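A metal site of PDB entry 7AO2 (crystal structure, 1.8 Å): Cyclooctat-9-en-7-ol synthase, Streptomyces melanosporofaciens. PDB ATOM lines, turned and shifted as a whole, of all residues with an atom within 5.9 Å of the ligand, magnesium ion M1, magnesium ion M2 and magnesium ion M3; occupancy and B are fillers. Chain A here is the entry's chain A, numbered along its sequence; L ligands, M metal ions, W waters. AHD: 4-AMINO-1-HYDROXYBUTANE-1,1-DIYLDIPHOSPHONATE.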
ATOM      1  N   ASN A 103      11.588   8.546  23.473  1.00  0.00           N
ATOM      2  CA  ASN A 103      10.477   9.350  22.937  1.00  0.00           C
ATOM      3  C   ASN A 103      10.544  10.781  23.437  1.00  0.00           C
ATOM      4  O   ASN A 103      10.447  11.729  22.645  1.00  0.00           O
ATOM      5  CB  ASN A 103       9.124   8.714  23.328  1.00  0.00           C
ATOM      6  CG  ASN A 103       7.932   9.597  22.991  1.00  0.00           C
ATOM      7  OD1 ASN A 103       7.400   9.511  21.859  1.00  0.00           O
ATOM      8  ND2 ASN A 103       7.451  10.419  23.974  1.00  0.00           N
ATOM      9  N   THR A 106      13.613  12.940  22.186  1.00  0.00           N
ATOM     10  CA  THR A 106      13.587  13.293  20.768  1.00  0.00           C
ATOM     11  C   THR A 106      12.399  14.175  20.423  1.00  0.00           C
ATOM     12  O   THR A 106      12.422  14.858  19.400  1.00  0.00           O
ATOM     13  CB  THR A 106      13.622  12.051  19.870  1.00  0.00           C
ATOM     14  OG1 THR A 106      12.500  11.199  20.147  1.00  0.00           O
ATOM     15  CG2 THR A 106      14.908  11.289  20.117  1.00  0.00           C
ATOM     16  N   PHE A 107      11.366  14.197  21.278  1.00  0.00           N
ATOM     17  CA  PHE A 107      10.350  15.235  21.155  1.00  0.00           C
ATOM     18  C   PHE A 107      10.953  16.620  21.372  1.00  0.00           C
ATOM     19  O   PHE A 107      10.577  17.579  20.694  1.00  0.00           O
ATOM     20  CB  PHE A 107       9.247  15.002  22.193  1.00  0.00           C
ATOM     21  CG  PHE A 107       7.944  14.511  21.641  1.00  0.00           C
ATOM     22  CD1 PHE A 107       7.056  15.381  20.995  1.00  0.00           C
ATOM     23  CD2 PHE A 107       7.565  13.179  21.822  1.00  0.00           C
ATOM     24  CE1 PHE A 107       5.816  14.952  20.543  1.00  0.00           C
ATOM     25  CE2 PHE A 107       6.319  12.712  21.324  1.00  0.00           C
ATOM     26  CZ  PHE A 107       5.434  13.612  20.688  1.00  0.00           C
ATOM     27  N   ASP A 110      12.530  17.533  18.209  1.00  0.00           N
ATOM     28  CA  ASP A 110      11.518  17.885  17.220  1.00  0.00           C
ATOM     29  C   ASP A 110      11.048  19.325  17.417  1.00  0.00           C
ATOM     30  O   ASP A 110      10.779  20.045  16.448  1.00  0.00           O
ATOM     31  CB  ASP A 110      10.343  16.896  17.367  1.00  0.00           C
ATOM     32  CG  ASP A 110       9.244  17.066  16.316  1.00  0.00           C
ATOM     33  OD1 ASP A 110       9.461  16.547  15.214  1.00  0.00           O
ATOM     34  OD2 ASP A 110       8.129  17.644  16.598  1.00  0.00           O
ATOM     35  N   ASP A 111      10.964  19.764  18.658  1.00  0.00           N
ATOM     36  CA  ASP A 111      10.465  21.095  18.947  1.00  0.00           C
ATOM     37  C   ASP A 111      11.543  22.172  18.858  1.00  0.00           C
ATOM     38  O   ASP A 111      11.203  23.361  18.969  1.00  0.00           O
ATOM     39  CB  ASP A 111       9.848  21.094  20.362  1.00  0.00           C
ATOM     40  CG  ASP A 111       8.423  20.539  20.369  1.00  0.00           C
ATOM     41  OD1 ASP A 111       7.806  20.485  19.287  1.00  0.00           O
ATOM     42  OD2 ASP A 111       7.929  20.129  21.446  1.00  0.00           O
ATOM     43  N   PHE A 149      16.407   8.949  13.503  1.00  0.00           N
ATOM     44  CA  PHE A 149      15.271   9.867  13.666  1.00  0.00           C
ATOM     45  C   PHE A 149      15.728  11.314  13.833  1.00  0.00           C
ATOM     46  O   PHE A 149      15.172  12.218  13.183  1.00  0.00           O
ATOM     47  CB  PHE A 149      14.393   9.455  14.864  1.00  0.00           C
ATOM     48  CG  PHE A 149      13.302  10.472  15.134  1.00  0.00           C
ATOM     49  CD1 PHE A 149      12.111  10.452  14.407  1.00  0.00           C
ATOM     50  CD2 PHE A 149      13.496  11.484  16.085  1.00  0.00           C
ATOM     51  CE1 PHE A 149      11.073  11.424  14.632  1.00  0.00           C
ATOM     52  CE2 PHE A 149      12.511  12.441  16.334  1.00  0.00           C
ATOM     53  CZ  PHE A 149      11.291  12.430  15.600  1.00  0.00           C
ATOM     54  N   ASP A 153      15.005  14.481  11.167  1.00  0.00           N
ATOM     55  CA  ASP A 153      14.337  15.723  11.507  1.00  0.00           C
ATOM     56  C   ASP A 153      15.224  16.929  11.203  1.00  0.00           C
ATOM     57  O   ASP A 153      14.752  17.962  10.727  1.00  0.00           O
ATOM     58  CB  ASP A 153      13.962  15.674  12.981  1.00  0.00           C
ATOM     59  CG  ASP A 153      13.406  16.976  13.440  1.00  0.00           C
ATOM     60  OD1 ASP A 153      12.384  17.424  12.891  1.00  0.00           O
ATOM     61  OD2 ASP A 153      13.995  17.550  14.362  1.00  0.00           O
ATOM     62  N   ARG A 177       6.595  10.152   6.053  1.00  0.00           N
ATOM     63  CA  ARG A 177       6.266  10.114   7.460  1.00  0.00           C
ATOM     64  C   ARG A 177       6.641   8.792   8.129  1.00  0.00           C
ATOM     65  O   ARG A 177       6.767   8.769   9.349  1.00  0.00           O
ATOM     66  CB  ARG A 177       4.772  10.414   7.634  1.00  0.00           C
ATOM     67  CG  ARG A 177       4.448  11.888   7.373  1.00  0.00           C
ATOM     68  CD  ARG A 177       5.104  12.834   8.413  1.00  0.00           C
ATOM     69  NE  ARG A 177       4.039  13.394   9.256  1.00  0.00           N
ATOM     70  CZ  ARG A 177       4.198  13.776  10.511  1.00  0.00           C
ATOM     71  NH1 ARG A 177       5.391  13.695  11.112  1.00  0.00           N
ATOM     72  NH2 ARG A 177       3.152  14.231  11.180  1.00  0.00           N
ATOM     73  N   ASP A 180       9.633  10.121   9.419  1.00  0.00           N
ATOM     74  CA  ASP A 180       9.673  11.454  10.032  1.00  0.00           C
ATOM     75  C   ASP A 180       8.788  11.540  11.274  1.00  0.00           C
ATOM     76  O   ASP A 180       9.137  12.209  12.250  1.00  0.00           O
ATOM     77  CB  ASP A 180       9.242  12.519   9.012  1.00  0.00           C
ATOM     78  CG  ASP A 180       9.134  13.912   9.634  1.00  0.00           C
ATOM     79  OD1 ASP A 180      10.180  14.587   9.794  1.00  0.00           O
ATOM     80  OD2 ASP A 180       8.005  14.326   9.977  1.00  0.00           O
ATOM     81  N   ILE A 181       7.636  10.870  11.261  1.00  0.00           N
ATOM     82  CA  ILE A 181       6.807  10.942  12.468  1.00  0.00           C
ATOM     83  C   ILE A 181       7.410  10.117  13.594  1.00  0.00           C
ATOM     84  O   ILE A 181       7.005  10.261  14.765  1.00  0.00           O
ATOM     85  CB  ILE A 181       5.376  10.479  12.164  1.00  0.00           C
ATOM     86  CG1 ILE A 181       4.411  11.005  13.273  1.00  0.00           C
ATOM     87  CG2 ILE A 181       5.292   8.909  12.027  1.00  0.00           C
ATOM     88  CD1 ILE A 181       2.935  10.877  12.941  1.00  0.00           C
ATOM     89  N   GLY A 182       8.358   9.223  13.280  1.00  0.00           N
ATOM     90  CA  GLY A 182       9.063   8.517  14.321  1.00  0.00           C
ATOM     91  C   GLY A 182       8.553   7.126  14.584  1.00  0.00           C
ATOM     92  O   GLY A 182       9.030   6.475  15.528  1.00  0.00           O
ATOM     93  N   ASN A 220      -2.433  12.414  14.252  1.00  0.00           N
ATOM     94  CA  ASN A 220      -1.558  13.491  14.688  1.00  0.00           C
ATOM     95  C   ASN A 220      -1.726  14.751  13.823  1.00  0.00           C
ATOM     96  O   ASN A 220      -1.790  15.865  14.346  1.00  0.00           O
ATOM     97  CB  ASN A 220      -0.099  13.083  14.672  1.00  0.00           C
ATOM     98  CG  ASN A 220       0.787  14.263  15.042  1.00  0.00           C
ATOM     99  OD1 ASN A 220       1.338  14.891  14.181  1.00  0.00           O
ATOM    100  ND2 ASN A 220       0.792  14.634  16.322  1.00  0.00           N
ATOM    101  N   ASP A 221      -1.803  14.597  12.504  1.00  0.00           N
ATOM    102  CA  ASP A 221      -1.917  15.769  11.648  1.00  0.00           C
ATOM    103  C   ASP A 221      -3.170  16.601  11.952  1.00  0.00           C
ATOM    104  O   ASP A 221      -3.134  17.846  11.941  1.00  0.00           O
ATOM    105  CB  ASP A 221      -1.909  15.336  10.185  1.00  0.00           C
ATOM    106  CG  ASP A 221      -0.552  14.843   9.719  1.00  0.00           C
ATOM    107  OD1 ASP A 221       0.422  14.962  10.502  1.00  0.00           O
ATOM    108  OD2 ASP A 221      -0.478  14.353   8.586  1.00  0.00           O
ATOM    109  N   SER A 224      -2.521  18.498  15.313  1.00  0.00           N
ATOM    110  CA  SER A 224      -1.374  19.417  15.370  1.00  0.00           C
ATOM    111  C   SER A 224      -1.381  20.422  14.214  1.00  0.00           C
ATOM    112  O   SER A 224      -0.467  21.254  14.119  1.00  0.00           O
ATOM    113  CB  SER A 224      -0.043  18.638  15.423  1.00  0.00           C
ATOM    114  OG  SER A 224       0.078  17.698  14.357  1.00  0.00           O
ATOM    115  N   TYR A 225      -2.421  20.395  13.367  1.00  0.00           N
ATOM    116  CA  TYR A 225      -2.494  21.294  12.209  1.00  0.00           C
ATOM    117  C   TYR A 225      -2.392  22.770  12.617  1.00  0.00           C
ATOM    118  O   TYR A 225      -1.620  23.539  12.011  1.00  0.00           O
ATOM    119  CB  TYR A 225      -3.812  21.060  11.471  1.00  0.00           C
ATOM    120  CG  TYR A 225      -3.988  21.927  10.232  1.00  0.00           C
ATOM    121  CD1 TYR A 225      -3.537  21.482   8.990  1.00  0.00           C
ATOM    122  CD2 TYR A 225      -4.632  23.179  10.292  1.00  0.00           C
ATOM    123  CE1 TYR A 225      -3.687  22.256   7.839  1.00  0.00           C
ATOM    124  CE2 TYR A 225      -4.792  23.988   9.117  1.00  0.00           C
ATOM    125  CZ  TYR A 225      -4.309  23.503   7.901  1.00  0.00           C
ATOM    126  OH  TYR A 225      -4.437  24.210   6.725  1.00  0.00           O
ATOM    127  N   ARG A 227      -1.239  24.370  15.253  1.00  0.00           N
ATOM    128  CA  ARG A 227       0.116  24.705  15.694  1.00  0.00           C
ATOM    129  C   ARG A 227       1.095  24.716  14.519  1.00  0.00           C
ATOM    130  O   ARG A 227       1.891  25.665  14.336  1.00  0.00           O
ATOM    131  CB  ARG A 227       0.601  23.727  16.782  1.00  0.00           C
ATOM    132  CG  ARG A 227       2.131  23.649  16.880  1.00  0.00           C
ATOM    133  CD  ARG A 227       2.664  22.935  18.090  1.00  0.00           C
ATOM    134  NE  ARG A 227       2.074  21.618  18.282  1.00  0.00           N
ATOM    135  CZ  ARG A 227       2.563  20.492  17.759  1.00  0.00           C
ATOM    136  NH1 ARG A 227       3.682  20.537  17.028  1.00  0.00           N
ATOM    137  NH2 ARG A 227       1.963  19.323  17.995  1.00  0.00           N
ATOM    138  N   GLU A 228       1.084  23.671  13.705  1.00  0.00           N
ATOM    139  CA  GLU A 228       2.092  23.557  12.659  1.00  0.00           C
ATOM    140  C   GLU A 228       1.922  24.645  11.605  1.00  0.00           C
ATOM    141  O   GLU A 228       2.903  25.300  11.211  1.00  0.00           O
ATOM    142  CB  GLU A 228       2.056  22.151  12.046  1.00  0.00           C
ATOM    143  CG  GLU A 228       2.633  21.159  13.062  1.00  0.00           C
ATOM    144  CD  GLU A 228       2.320  19.697  12.760  1.00  0.00           C
ATOM    145  OE1 GLU A 228       1.734  19.417  11.681  1.00  0.00           O
ATOM    146  OE2 GLU A 228       2.704  18.856  13.591  1.00  0.00           O
ATOM    147  N   GLN A 233       5.272  25.090   9.470  1.00  0.00           N
ATOM    148  CA  GLN A 233       5.641  23.687   9.312  1.00  0.00           C
ATOM    149  C   GLN A 233       4.734  23.027   8.258  1.00  0.00           C
ATOM    150  O   GLN A 233       3.514  23.089   8.337  1.00  0.00           O
ATOM    151  CB  GLN A 233       5.544  23.006  10.678  1.00  0.00           C
ATOM    152  CG  GLN A 233       6.702  23.476  11.581  1.00  0.00           C
ATOM    153  CD  GLN A 233       6.587  22.903  12.968  1.00  0.00           C
ATOM    154  OE1 GLN A 233       5.509  22.924  13.550  1.00  0.00           O
ATOM    155  NE2 GLN A 233       7.689  22.351  13.498  1.00  0.00           N
ATOM    156  N   THR A 235       4.795  19.729   7.215  1.00  0.00           N
ATOM    157  CA  THR A 235       4.654  18.273   7.275  1.00  0.00           C
ATOM    158  C   THR A 235       3.307  17.950   7.931  1.00  0.00           C
ATOM    159  O   THR A 235       3.209  17.574   9.112  1.00  0.00           O
ATOM    160  CB  THR A 235       5.838  17.651   8.029  1.00  0.00           C
ATOM    161  OG1 THR A 235       7.074  18.126   7.461  1.00  0.00           O
ATOM    162  CG2 THR A 235       5.825  16.111   7.966  1.00  0.00           C
ATOM    163  N   ASN A 236       2.237  18.055   7.130  1.00  0.00           N
ATOM    164  CA  ASN A 236       0.884  17.799   7.655  1.00  0.00           C
ATOM    165  C   ASN A 236      -0.034  17.498   6.473  1.00  0.00           C
ATOM    166  O   ASN A 236      -0.182  18.349   5.583  1.00  0.00           O
ATOM    167  CB  ASN A 236       0.396  19.002   8.439  1.00  0.00           C
ATOM    168  CG  ASN A 236      -0.910  18.718   9.161  1.00  0.00           C
ATOM    169  OD1 ASN A 236      -1.900  18.309   8.539  1.00  0.00           O
ATOM    170  ND2 ASN A 236      -0.915  18.904  10.508  1.00  0.00           N
ATOM    171  N   ARG A 294      -0.764  19.290  24.671  1.00  0.00           N
ATOM    172  CA  ARG A 294       0.002  19.619  23.476  1.00  0.00           C
ATOM    173  C   ARG A 294      -0.902  19.823  22.254  1.00  0.00           C
ATOM    174  O   ARG A 294      -0.588  20.630  21.367  1.00  0.00           O
ATOM    175  CB  ARG A 294       1.028  18.516  23.213  1.00  0.00           C
ATOM    176  CG  ARG A 294       1.804  18.720  21.889  1.00  0.00           C
ATOM    177  CD  ARG A 294       2.941  17.707  21.798  1.00  0.00           C
ATOM    178  NE  ARG A 294       3.809  17.925  20.622  1.00  0.00           N
ATOM    179  CZ  ARG A 294       4.874  18.734  20.586  1.00  0.00           C
ATOM    180  NH1 ARG A 294       5.219  19.453  21.646  1.00  0.00           N
ATOM    181  NH2 ARG A 294       5.622  18.827  19.484  1.00  0.00           N
ATOM    182  N   TYR A 295      -2.016  19.113  22.164  1.00  0.00           N
ATOM    183  CA  TYR A 295      -2.774  19.050  20.917  1.00  0.00           C
ATOM    184  C   TYR A 295      -4.109  19.785  21.020  1.00  0.00           C
ATOM    185  O   TYR A 295      -5.147  19.324  20.506  1.00  0.00           O
ATOM    186  CB  TYR A 295      -2.941  17.603  20.489  1.00  0.00           C
ATOM    187  CG  TYR A 295      -1.628  16.918  20.271  1.00  0.00           C
ATOM    188  CD1 TYR A 295      -0.811  17.303  19.193  1.00  0.00           C
ATOM    189  CD2 TYR A 295      -1.208  15.861  21.084  1.00  0.00           C
ATOM    190  CE1 TYR A 295       0.405  16.697  18.952  1.00  0.00           C
ATOM    191  CE2 TYR A 295       0.022  15.230  20.867  1.00  0.00           C
ATOM    192  CZ  TYR A 295       0.809  15.654  19.777  1.00  0.00           C
ATOM    193  OH  TYR A 295       1.997  15.077  19.516  1.00  0.00           O
HETATM  194  C2  AHD L   1       6.500  13.358  16.673  1.00  0.00           C
HETATM  195  C3  AHD L   1       7.440  12.733  17.727  1.00  0.00           C
HETATM  196  C7  AHD L   1       6.015  14.820  16.999  1.00  0.00           C
HETATM  197  C8  AHD L   1       4.773  15.159  16.133  1.00  0.00           C
HETATM  198  O12 AHD L   1       3.620  16.417  18.261  1.00  0.00           O
HETATM  199  P9  AHD L   1       3.955  16.662  16.805  1.00  0.00           P
HETATM  200  O10 AHD L   1       2.724  17.038  16.034  1.00  0.00           O
HETATM  201  O11 AHD L   1       4.956  17.782  16.664  1.00  0.00           O
HETATM  202  P14 AHD L   1       5.233  15.451  14.370  1.00  0.00           P
HETATM  203  O15 AHD L   1       6.415  16.425  14.359  1.00  0.00           O
HETATM  204  O16 AHD L   1       4.090  16.071  13.629  1.00  0.00           O
HETATM  205  O17 AHD L   1       5.700  14.104  13.782  1.00  0.00           O
HETATM  206  O13 AHD L   1       3.815  14.136  16.098  1.00  0.00           O
HETATM  207  N4  AHD L   1       7.686  11.327  17.379  1.00  0.00           N
HETATM  208 MG    MG M   1       2.197  16.920  14.062  1.00  0.00          MG
HETATM  209 MG    MG M   2       6.577  18.240  15.473  1.00  0.00          MG
HETATM  210 MG    MG M   3       8.367  16.285  13.544  1.00  0.00          MG
HETATM  211  O   HOH W   1       8.266  14.234  13.770  1.00  0.00           O
HETATM  212  O   HOH W   2       5.342  19.436  14.278  1.00  0.00           O
HETATM  213  O   HOH W   3      10.120  16.117  12.343  1.00  0.00           O
HETATM  214  O   HOH W   4       1.593  16.691  11.931  1.00  0.00           O
HETATM  215  O   HOH W   5       7.422  16.352  11.659  1.00  0.00           O
HETATM  216  O   HOH W   6       8.121  18.455  13.645  1.00  0.00           O
HETATM  217  O   HOH W   7       4.914  17.334  11.338  1.00  0.00           O
HETATM  218  O   HOH W   8       7.146  20.053  16.373  1.00  0.00           O
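The side-chain hydroxyl (OH) of Tyr 295 sits at hydrogen-bond distance from an oxygen (O12) of the ligand (2.5 Å). An oxygen (O12) of the ligand is in salt-bridge range of the guanidinium group (NH2) of Arg 227 (3.4 Å). The guanidinium group (NH1) of Arg 177 is in salt-bridge range of an oxygen (O17) of the ligand, at 2.7 Å. The backbone carbonyl oxygen (O) of Ile 181 lies within hydrogen-bond range of a nitrogen (N4) of the ligand. NE of Arg 294 is in salt-bridge range of O12 of the ligand.
The side-chain amide nitrogen (ND2) of Asn 236 sits at hydrogen-bond distance from the side-chain carboxylate (OE1) of Glu 228. OH of Tyr 295 sits close to ND2 of Asn 220. The guanidinium group (NH2) of Arg 177 lies within salt-bridge range of the side-chain carboxylate (OD1) of Asp 221. The guanidinium group of Arg 227 lies close to the side-chain carboxylate of Glu 228, 3.9 Å away. The side-chain carboxylate (OD1) of Asp 111 is in salt-bridge range of the guanidinium group (NH2) of Arg 294, 2.7 Å away. The guanidinium group (NH1) of Arg 177 is in salt-bridge range of the side-chain carboxylate (OD2) of Asp 180, at 2.9 Å. N of Gln 233 sits at hydrogen-bond distance from O of Glu 228.
CE1 of Phe 107 touches O12 of the ligand (3.5 Å). Hydrophobic or aromatic side chains that line the ligand: Phe 107, Ile 181 and Tyr 295. Within 4 Å of the ligand: Phe 107, Asp 110, Arg 177, Ile 181, Asn 220, Ser 224, Arg 227, Glu 228, Arg 294 and Tyr 295. The nearest printed residue that does not touch the ligand is Phe 149 (4.2 Å).
Of the 22 residues printed, 3 come within 4 Å of magnesium ion M1.
Of the 22 residues printed, 1 comes within 4 Å of magnesium ion M2. The nearest printed residue that does not touch magnesium ion M2 is Arg 227 (4.01 Å).
Within 4 Å of magnesium ion M3: Asp 110.
Magnesium ion M1 is bound by O10 of the ligand (2.0 Å), OE2 of Glu 228 (2.1 Å), O16 of the ligand (2.1 Å), OD1 of Asn 220 (2.2 Å), water W4 (2.2 Å) and OG of Ser 224 (2.3 Å). Magnesium ion M1 has six donor atoms within binding distance.
Magnesium ion M2 is bound by OD2 of Asp 110, at 2.0 Å. O11 of the ligand binds magnesium ion M2, 2.1 Å away. Water W2 binds magnesium ion M2, 2.1 Å away. Water W8 is bound to magnesium ion M2. Magnesium ion M2 is bound by O15 of the ligand (2.1 Å). Magnesium ion M2 is bound by water W6, at 2.4 Å.
Magnesium ion M3 is bound by the side-chain carboxylate (OD1) of Asp 110 (2.0 Å), water W1 (2.1 Å), water W5 (2.1 Å), an oxygen (O15) of the ligand (2.1 Å), water W3 (2.1 Å) and water W6 (2.2 Å). Magnesium ion M3 has six donor atoms within binding distance.
Water W3 lies within hydrogen-bond range of OD1 of Asp 153 (2.7 Å) and OD1 of Asp 180 (3.0 Å). Water W1 lies within hydrogen-bond range of O17 of the ligand (2.6 Å) and O of Asp 180 (2.7 Å). Water W5 bridges the side-chain carboxylate (OD2) of Asp 180 and the guanidinium group (NH1) of Arg 177.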
